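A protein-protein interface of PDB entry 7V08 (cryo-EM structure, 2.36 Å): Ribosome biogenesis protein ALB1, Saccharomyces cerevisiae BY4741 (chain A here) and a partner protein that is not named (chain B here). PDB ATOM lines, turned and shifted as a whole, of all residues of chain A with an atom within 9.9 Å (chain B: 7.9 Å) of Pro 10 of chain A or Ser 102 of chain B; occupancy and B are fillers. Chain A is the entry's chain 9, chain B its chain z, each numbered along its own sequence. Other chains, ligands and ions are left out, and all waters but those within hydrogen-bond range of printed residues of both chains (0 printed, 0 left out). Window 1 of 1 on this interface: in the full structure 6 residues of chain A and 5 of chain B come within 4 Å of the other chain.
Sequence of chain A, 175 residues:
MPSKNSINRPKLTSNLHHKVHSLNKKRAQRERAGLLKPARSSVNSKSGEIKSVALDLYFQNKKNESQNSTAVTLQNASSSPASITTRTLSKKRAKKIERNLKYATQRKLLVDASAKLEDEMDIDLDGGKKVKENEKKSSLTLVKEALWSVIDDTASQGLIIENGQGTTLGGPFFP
The backbone carbonyl oxygen (O) of Gln 96 of chain B sits at hydrogen-bond distance from the backbone NH (N) of Thr 101 of chain B, 3.0 Å away.
The backbone NH (N) of Thr 104 of chain B sits at hydrogen-bond distance from the side-chain hydroxyl (OG) of Ser 102 of chain B (3.2 Å).
The backbone NH (N) of Arg 105 of chain B sits at hydrogen-bond distance from the side-chain hydroxyl (OG) of Ser 102 of chain B (2.8 Å).
O of Pro 10 of chain A sits at hydrogen-bond distance from OG of Ser 14 of chain A, 3.3 Å away.
OG of Ser 14 of chain A is in hydrogen-bond range of O of Lys 11 of chain A (2.7 Å).
Printed residues of chain A that touch a printed residue of chain B: Ser 6, Asn 8, Arg 9, Pro 10, Ser 14 and His 17.
NE2 of His 17 of chain A sits close to NZ of Lys 100 of chain B, 3.4 Å away.
The backbone carbonyl oxygen (O) of Ser 102 of chain B lies close to the backbone carbonyl oxygen (O) of Asn 8 of chain A (3.4 Å).
Of the printed residues of chain B, Asn 8 of chain A touches Ser 102 (3.4 Å) and Phe 103 (3.2 Å).
Of chain B, only Lys 100 (3.8 Å) and Ser 102 (3.6 Å) come within 4 Å of Pro 10 of chain A.
Of the printed residues of chain A, Lys 100 of chain B touches Pro 10 (3.8 Å), Ser 14 (3.7 Å) and His 17 (3.3 Å).
Of chain A, only Arg 9 (3.7 Å) comes within 4 Å of Thr 101 of chain B.
No residue of chain A comes within 4 Å of Thr 104 of chain B.
Among the printed residues, pairs that only touch across the chains: Asn 8 of chain A with Phe 103 of chain B (3.2 Å), Ser 14 of chain A with Lys 99 of chain B (3.3 Å), Ser 6 of chain A with Phe 103 of chain B (3.5 Å), Pro 10 of chain A with Ser 102 of chain B (3.6 Å), Ser 14 of chain A with Lys 100 of chain B (3.7 Å), Arg 9 of chain A with Thr 101 of chain B (3.7 Å), Pro 10 of chain A with Lys 100 of chain B (3.8 Å), Arg 9 of chain A with Phe 103 of chain B (3.8 Å) and Arg 9 of chain A with Ser 102 of chain B (3.9 Å).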
ATOM      1  N   PRO A   2       2.121  -5.869  17.365  1.00  0.00           N
ATOM      2  CA  PRO A   2       3.486  -6.356  17.146  1.00  0.00           C
ATOM      3  C   PRO A   2       4.363  -6.270  18.394  1.00  0.00           C
ATOM      4  O   PRO A   2       3.994  -5.634  19.381  1.00  0.00           O
ATOM      5  CB  PRO A   2       4.010  -5.427  16.055  1.00  0.00           C
ATOM      6  CG  PRO A   2       3.271  -4.168  16.272  1.00  0.00           C
ATOM      7  CD  PRO A   2       1.897  -4.564  16.725  1.00  0.00           C
ATOM      8  N   SER A   3       5.515  -6.925  18.335  1.00  0.00           N
ATOM      9  CA  SER A   3       6.460  -6.905  19.439  1.00  0.00           C
ATOM     10  C   SER A   3       7.227  -5.588  19.465  1.00  0.00           C
ATOM     11  O   SER A   3       7.366  -4.907  18.449  1.00  0.00           O
ATOM     12  CB  SER A   3       7.429  -8.081  19.315  1.00  0.00           C
ATOM     13  OG  SER A   3       8.364  -8.093  20.373  1.00  0.00           O
ATOM     14  N   SER A   6      10.558  -6.126  17.489  1.00  0.00           N
ATOM     15  CA  SER A   6      10.477  -6.192  16.030  1.00  0.00           C
ATOM     16  C   SER A   6       9.144  -5.582  15.604  1.00  0.00           C
ATOM     17  O   SER A   6       8.162  -6.305  15.420  1.00  0.00           O
ATOM     18  CB  SER A   6      10.620  -7.628  15.552  1.00  0.00           C
ATOM     19  OG  SER A   6       9.741  -8.490  16.250  1.00  0.00           O
ATOM     20  N   ILE A   7       9.129  -4.266  15.396  1.00  0.00           N
ATOM     21  CA  ILE A   7       7.870  -3.584  15.114  1.00  0.00           C
ATOM     22  C   ILE A   7       7.407  -3.764  13.675  1.00  0.00           C
ATOM     23  O   ILE A   7       6.199  -3.692  13.413  1.00  0.00           O
ATOM     24  CB  ILE A   7       7.955  -2.078  15.426  1.00  0.00           C
ATOM     25  CG1 ILE A   7       9.134  -1.439  14.695  1.00  0.00           C
ATOM     26  CG2 ILE A   7       8.050  -1.841  16.914  1.00  0.00           C
ATOM     27  CD1 ILE A   7       9.041   0.050  14.629  1.00  0.00           C
ATOM     28  N   ASN A   8       8.321  -4.004  12.739  1.00  0.00           N
ATOM     29  CA  ASN A   8       7.964  -4.146  11.337  1.00  0.00           C
ATOM     30  C   ASN A   8       7.470  -5.543  10.981  1.00  0.00           C
ATOM     31  O   ASN A   8       6.992  -5.740   9.860  1.00  0.00           O
ATOM     32  CB  ASN A   8       9.161  -3.774  10.455  1.00  0.00           C
ATOM     33  CG  ASN A   8       9.432  -2.276  10.436  1.00  0.00           C
ATOM     34  OD1 ASN A   8       8.514  -1.464  10.494  1.00  0.00           O
ATOM     35  ND2 ASN A   8      10.699  -1.909  10.354  1.00  0.00           N
ATOM     36  N   ARG A   9       7.553  -6.508  11.897  1.00  0.00           N
ATOM     37  CA  ARG A   9       7.103  -7.867  11.622  1.00  0.00           C
ATOM     38  C   ARG A   9       5.743  -8.108  12.258  1.00  0.00           C
ATOM     39  O   ARG A   9       5.608  -7.963  13.480  1.00  0.00           O
ATOM     40  CB  ARG A   9       8.115  -8.894  12.129  1.00  0.00           C
ATOM     41  CG  ARG A   9       7.720 -10.336  11.845  1.00  0.00           C
ATOM     42  CD  ARG A   9       8.857 -11.297  12.135  1.00  0.00           C
ATOM     43  NE  ARG A   9       9.263 -11.254  13.534  1.00  0.00           N
ATOM     44  CZ  ARG A   9      10.244 -11.977  14.051  1.00  0.00           C
ATOM     45  NH1 ARG A   9      10.952 -12.809  13.307  1.00  0.00           N
ATOM     46  NH2 ARG A   9      10.523 -11.861  15.344  1.00  0.00           N
ATOM     47  N   PRO A  10       4.717  -8.464  11.480  1.00  0.00           N
ATOM     48  CA  PRO A  10       3.414  -8.780  12.074  1.00  0.00           C
ATOM     49  C   PRO A  10       3.478 -10.043  12.916  1.00  0.00           C
ATOM     50  O   PRO A  10       4.121 -11.029  12.551  1.00  0.00           O
ATOM     51  CB  PRO A  10       2.503  -8.970  10.856  1.00  0.00           C
ATOM     52  CG  PRO A  10       3.251  -8.401   9.709  1.00  0.00           C
ATOM     53  CD  PRO A  10       4.689  -8.595  10.018  1.00  0.00           C
ATOM     54  N   LYS A  11       2.816  -9.989  14.068  1.00  0.00           N
ATOM     55  CA  LYS A  11       2.850 -11.064  15.049  1.00  0.00           C
ATOM     56  C   LYS A  11       1.471 -11.662  15.292  1.00  0.00           C
ATOM     57  O   LYS A  11       1.271 -12.864  15.065  1.00  0.00           O
ATOM     58  CB  LYS A  11       3.453 -10.503  16.341  1.00  0.00           C
ATOM     59  CG  LYS A  11       3.756 -11.506  17.412  1.00  0.00           C
ATOM     60  CD  LYS A  11       4.423 -10.810  18.571  1.00  0.00           C
ATOM     61  CE  LYS A  11       4.508 -11.705  19.766  1.00  0.00           C
ATOM     62  NZ  LYS A  11       5.141 -13.004  19.436  1.00  0.00           N
ATOM     63  N   LEU A  12       0.501 -10.840  15.710  1.00  0.00           N
ATOM     64  CA  LEU A  12      -0.847 -11.328  15.979  1.00  0.00           C
ATOM     65  C   LEU A  12      -1.524 -11.825  14.709  1.00  0.00           C
ATOM     66  O   LEU A  12      -2.180 -12.869  14.727  1.00  0.00           O
ATOM     67  CB  LEU A  12      -1.680 -10.228  16.648  1.00  0.00           C
ATOM     68  CG  LEU A  12      -3.192 -10.427  16.825  1.00  0.00           C
ATOM     69  CD1 LEU A  12      -3.521 -11.649  17.666  1.00  0.00           C
ATOM     70  CD2 LEU A  12      -3.852  -9.195  17.425  1.00  0.00           C
ATOM     71  N   THR A  13      -1.366 -11.105  13.596  1.00  0.00           N
ATOM     72  CA  THR A  13      -1.977 -11.533  12.340  1.00  0.00           C
ATOM     73  C   THR A  13      -1.390 -12.854  11.852  1.00  0.00           C
ATOM     74  O   THR A  13      -2.122 -13.714  11.348  1.00  0.00           O
ATOM     75  CB  THR A  13      -1.820 -10.449  11.270  1.00  0.00           C
ATOM     76  OG1 THR A  13      -0.483  -9.945  11.284  1.00  0.00           O
ATOM     77  CG2 THR A  13      -2.768  -9.312  11.525  1.00  0.00           C
ATOM     78  N   SER A  14      -0.075 -13.034  11.992  1.00  0.00           N
ATOM     79  CA  SER A  14       0.541 -14.294  11.590  1.00  0.00           C
ATOM     80  C   SER A  14       0.053 -15.450  12.461  1.00  0.00           C
ATOM     81  O   SER A  14      -0.254 -16.538  11.952  1.00  0.00           O
ATOM     82  CB  SER A  14       2.065 -14.171  11.636  1.00  0.00           C
ATOM     83  OG  SER A  14       2.531 -13.847  12.936  1.00  0.00           O
ATOM     84  N   ASN A  15      -0.057 -15.218  13.775  1.00  0.00           N
ATOM     85  CA  ASN A  15      -0.583 -16.248  14.668  1.00  0.00           C
ATOM     86  C   ASN A  15      -2.031 -16.591  14.333  1.00  0.00           C
ATOM     87  O   ASN A  15      -2.417 -17.766  14.357  1.00  0.00           O
ATOM     88  CB  ASN A  15      -0.472 -15.797  16.124  1.00  0.00           C
ATOM     89  CG  ASN A  15       0.960 -15.581  16.564  1.00  0.00           C
ATOM     90  OD1 ASN A  15       1.885 -16.175  16.019  1.00  0.00           O
ATOM     91  ND2 ASN A  15       1.147 -14.726  17.563  1.00  0.00           N
ATOM     92  N   LEU A  16      -2.845 -15.578  14.026  1.00  0.00           N
ATOM     93  CA  LEU A  16      -4.242 -15.811  13.673  1.00  0.00           C
ATOM     94  C   LEU A  16      -4.365 -16.597  12.377  1.00  0.00           C
ATOM     95  O   LEU A  16      -5.216 -17.486  12.263  1.00  0.00           O
ATOM     96  CB  LEU A  16      -4.991 -14.484  13.545  1.00  0.00           C
ATOM     97  CG  LEU A  16      -5.299 -13.645  14.781  1.00  0.00           C
ATOM     98  CD1 LEU A  16      -6.156 -12.452  14.388  1.00  0.00           C
ATOM     99  CD2 LEU A  16      -5.978 -14.478  15.851  1.00  0.00           C
ATOM    100  N   HIS A  17      -3.540 -16.264  11.383  1.00  0.00           N
ATOM    101  CA  HIS A  17      -3.570 -16.981  10.114  1.00  0.00           C
ATOM    102  C   HIS A  17      -3.221 -18.450  10.315  1.00  0.00           C
ATOM    103  O   HIS A  17      -3.903 -19.347   9.791  1.00  0.00           O
ATOM    104  CB  HIS A  17      -2.603 -16.317   9.136  1.00  0.00           C
ATOM    105  CG  HIS A  17      -2.817 -16.704   7.709  1.00  0.00           C
ATOM    106  ND1 HIS A  17      -3.914 -16.293   6.984  1.00  0.00           N
ATOM    107  CD2 HIS A  17      -2.069 -17.454   6.869  1.00  0.00           C
ATOM    108  CE1 HIS A  17      -3.832 -16.776   5.758  1.00  0.00           C
ATOM    109  NE2 HIS A  17      -2.723 -17.486   5.664  1.00  0.00           N
ATOM    110  N   LEU B  93      12.088 -16.753   1.533  1.00  0.00           N
ATOM    111  CA  LEU B  93      11.265 -15.588   1.214  1.00  0.00           C
ATOM    112  C   LEU B  93       9.831 -15.989   0.898  1.00  0.00           C
ATOM    113  O   LEU B  93       8.886 -15.297   1.299  1.00  0.00           O
ATOM    114  CB  LEU B  93      11.878 -14.810   0.054  1.00  0.00           C
ATOM    115  CG  LEU B  93      13.223 -14.176   0.404  1.00  0.00           C
ATOM    116  CD1 LEU B  93      13.836 -13.536  -0.812  1.00  0.00           C
ATOM    117  CD2 LEU B  93      13.065 -13.167   1.525  1.00  0.00           C
ATOM    118  N   LYS B  95       8.336 -18.627   2.174  1.00  0.00           N
ATOM    119  CA  LYS B  95       7.767 -18.985   3.468  1.00  0.00           C
ATOM    120  C   LYS B  95       7.368 -17.749   4.265  1.00  0.00           C
ATOM    121  O   LYS B  95       6.318 -17.737   4.917  1.00  0.00           O
ATOM    122  CB  LYS B  95       8.764 -19.828   4.260  1.00  0.00           C
ATOM    123  CG  LYS B  95       8.231 -20.307   5.596  1.00  0.00           C
ATOM    124  CD  LYS B  95       9.343 -20.704   6.545  1.00  0.00           C
ATOM    125  CE  LYS B  95      10.083 -21.932   6.051  1.00  0.00           C
ATOM    126  NZ  LYS B  95      11.336 -22.168   6.813  1.00  0.00           N
ATOM    127  N   GLN B  96       8.203 -16.705   4.241  1.00  0.00           N
ATOM    128  CA  GLN B  96       7.869 -15.475   4.954  1.00  0.00           C
ATOM    129  C   GLN B  96       6.645 -14.805   4.348  1.00  0.00           C
ATOM    130  O   GLN B  96       5.796 -14.281   5.078  1.00  0.00           O
ATOM    131  CB  GLN B  96       9.062 -14.521   4.973  1.00  0.00           C
ATOM    132  CG  GLN B  96      10.155 -14.939   5.946  1.00  0.00           C
ATOM    133  CD  GLN B  96      11.331 -13.987   5.949  1.00  0.00           C
ATOM    134  OE1 GLN B  96      11.249 -12.878   5.424  1.00  0.00           O
ATOM    135  NE2 GLN B  96      12.437 -14.418   6.540  1.00  0.00           N
ATOM    136  N   SER B  97       6.527 -14.834   3.019  1.00  0.00           N
ATOM    137  CA  SER B  97       5.311 -14.345   2.380  1.00  0.00           C
ATOM    138  C   SER B  97       4.089 -15.140   2.825  1.00  0.00           C
ATOM    139  O   SER B  97       3.044 -14.563   3.149  1.00  0.00           O
ATOM    140  CB  SER B  97       5.453 -14.411   0.864  1.00  0.00           C
ATOM    141  OG  SER B  97       4.183 -14.552   0.254  1.00  0.00           O
ATOM    142  N   LYS B  98       4.206 -16.467   2.863  1.00  0.00           N
ATOM    143  CA  LYS B  98       3.050 -17.306   3.149  1.00  0.00           C
ATOM    144  C   LYS B  98       2.604 -17.170   4.601  1.00  0.00           C
ATOM    145  O   LYS B  98       1.404 -17.086   4.881  1.00  0.00           O
ATOM    146  CB  LYS B  98       3.376 -18.760   2.811  1.00  0.00           C
ATOM    147  CG  LYS B  98       2.192 -19.697   2.877  1.00  0.00           C
ATOM    148  CD  LYS B  98       1.074 -19.245   1.959  1.00  0.00           C
ATOM    149  CE  LYS B  98      -0.101 -20.189   2.057  1.00  0.00           C
ATOM    150  NZ  LYS B  98      -0.533 -20.383   3.469  1.00  0.00           N
ATOM    151  N   LYS B  99       3.551 -17.131   5.532  1.00  0.00           N
ATOM    152  CA  LYS B  99       3.255 -17.019   6.951  1.00  0.00           C
ATOM    153  C   LYS B  99       3.100 -15.580   7.425  1.00  0.00           C
ATOM    154  O   LYS B  99       2.814 -15.372   8.609  1.00  0.00           O
ATOM    155  CB  LYS B  99       4.350 -17.710   7.767  1.00  0.00           C
ATOM    156  CG  LYS B  99       4.375 -19.219   7.621  1.00  0.00           C
ATOM    157  CD  LYS B  99       5.691 -19.786   8.114  1.00  0.00           C
ATOM    158  CE  LYS B  99       5.681 -21.303   8.159  1.00  0.00           C
ATOM    159  NZ  LYS B  99       4.867 -21.819   9.289  1.00  0.00           N
ATOM    160  N   LYS B 100       3.284 -14.593   6.538  1.00  0.00           N
ATOM    161  CA  LYS B 100       3.162 -13.173   6.880  1.00  0.00           C
ATOM    162  C   LYS B 100       4.149 -12.783   7.980  1.00  0.00           C
ATOM    163  O   LYS B 100       3.770 -12.216   9.007  1.00  0.00           O
ATOM    164  CB  LYS B 100       1.730 -12.814   7.283  1.00  0.00           C
ATOM    165  CG  LYS B 100       0.663 -13.228   6.279  1.00  0.00           C
ATOM    166  CD  LYS B 100      -0.693 -13.286   6.955  1.00  0.00           C
ATOM    167  CE  LYS B 100      -1.822 -13.207   5.952  1.00  0.00           C
ATOM    168  NZ  LYS B 100      -1.792 -14.316   4.972  1.00  0.00           N
ATOM    169  N   THR B 101       5.423 -13.103   7.776  1.00  0.00           N
ATOM    170  CA  THR B 101       6.473 -12.857   8.759  1.00  0.00           C
ATOM    171  C   THR B 101       7.607 -12.028   8.175  1.00  0.00           C
ATOM    172  O   THR B 101       8.775 -12.209   8.524  1.00  0.00           O
ATOM    173  CB  THR B 101       7.023 -14.171   9.308  1.00  0.00           C
ATOM    174  OG1 THR B 101       7.200 -15.098   8.231  1.00  0.00           O
ATOM    175  CG2 THR B 101       6.087 -14.762  10.341  1.00  0.00           C
ATOM    176  N   SER B 102       7.285 -11.093   7.294  1.00  0.00           N
ATOM    177  CA  SER B 102       8.295 -10.292   6.623  1.00  0.00           C
ATOM    178  C   SER B 102       8.491  -8.970   7.352  1.00  0.00           C
ATOM    179  O   SER B 102       7.524  -8.337   7.780  1.00  0.00           O
ATOM    180  CB  SER B 102       7.910 -10.031   5.168  1.00  0.00           C
ATOM    181  OG  SER B 102       8.800  -9.113   4.563  1.00  0.00           O
ATOM    182  N   PHE B 103       9.754  -8.567   7.493  1.00  0.00           N
ATOM    183  CA  PHE B 103      10.080  -7.271   8.077  1.00  0.00           C
ATOM    184  C   PHE B 103       9.840  -6.126   7.100  1.00  0.00           C
ATOM    185  O   PHE B 103       9.583  -4.993   7.518  1.00  0.00           O
ATOM    186  CB  PHE B 103      11.532  -7.260   8.548  1.00  0.00           C
ATOM    187  CG  PHE B 103      11.730  -7.873   9.892  1.00  0.00           C
ATOM    188  CD1 PHE B 103      11.619  -7.104  11.033  1.00  0.00           C
ATOM    189  CD2 PHE B 103      12.028  -9.219  10.020  1.00  0.00           C
ATOM    190  CE1 PHE B 103      11.791  -7.660  12.274  1.00  0.00           C
ATOM    191  CE2 PHE B 103      12.200  -9.783  11.265  1.00  0.00           C
ATOM    192  CZ  PHE B 103      12.085  -9.003  12.395  1.00  0.00           C
ATOM    193  N   THR B 104       9.946  -6.388   5.802  1.00  0.00           N
ATOM    194  CA  THR B 104       9.916  -5.324   4.815  1.00  0.00           C
ATOM    195  C   THR B 104       8.820  -5.465   3.773  1.00  0.00           C
ATOM    196  O   THR B 104       8.658  -4.558   2.955  1.00  0.00           O
ATOM    197  CB  THR B 104      11.269  -5.233   4.092  1.00  0.00           C
ATOM    198  OG1 THR B 104      11.774  -6.550   3.844  1.00  0.00           O
ATOM    199  CG2 THR B 104      12.267  -4.468   4.930  1.00  0.00           C
ATOM    200  N   ARG B 105       8.075  -6.563   3.768  1.00  0.00           N
ATOM    201  CA  ARG B 105       7.054  -6.793   2.757  1.00  0.00           C
ATOM    202  C   ARG B 105       5.744  -7.200   3.411  1.00  0.00           C
ATOM    203  O   ARG B 105       5.722  -7.666   4.555  1.00  0.00           O
ATOM    204  CB  ARG B 105       7.505  -7.857   1.754  1.00  0.00           C
ATOM    205  CG  ARG B 105       8.733  -7.443   0.975  1.00  0.00           C
ATOM    206  CD  ARG B 105       9.300  -8.568   0.142  1.00  0.00           C
ATOM    207  NE  ARG B 105      10.335  -8.076  -0.758  1.00  0.00           N
ATOM    208  CZ  ARG B 105      10.090  -7.483  -1.918  1.00  0.00           C
ATOM    209  NH1 ARG B 105       8.853  -7.294  -2.348  1.00  0.00           N
ATOM    210  NH2 ARG B 105      11.110  -7.068  -2.665  1.00  0.00           N
ATOM    211  N   PHE B 106       4.654  -6.996   2.686  1.00  0.00           N
ATOM    212  CA  PHE B 106       3.337  -7.378   3.161  1.00  0.00           C
ATOM    213  C   PHE B 106       2.851  -8.637   2.446  1.00  0.00           C
ATOM    214  O   PHE B 106       2.943  -8.743   1.225  1.00  0.00           O
ATOM    215  CB  PHE B 106       2.340  -6.235   2.960  1.00  0.00           C
ATOM    216  CG  PHE B 106       2.536  -5.075   3.903  1.00  0.00           C
ATOM    217  CD1 PHE B 106       2.123  -5.160   5.222  1.00  0.00           C
ATOM    218  CD2 PHE B 106       3.111  -3.901   3.462  1.00  0.00           C
ATOM    219  CE1 PHE B 106       2.289  -4.089   6.085  1.00  0.00           C
ATOM    220  CE2 PHE B 106       3.275  -2.832   4.316  1.00  0.00           C
ATOM    221  CZ  PHE B 106       2.862  -2.923   5.630  1.00  0.00           C
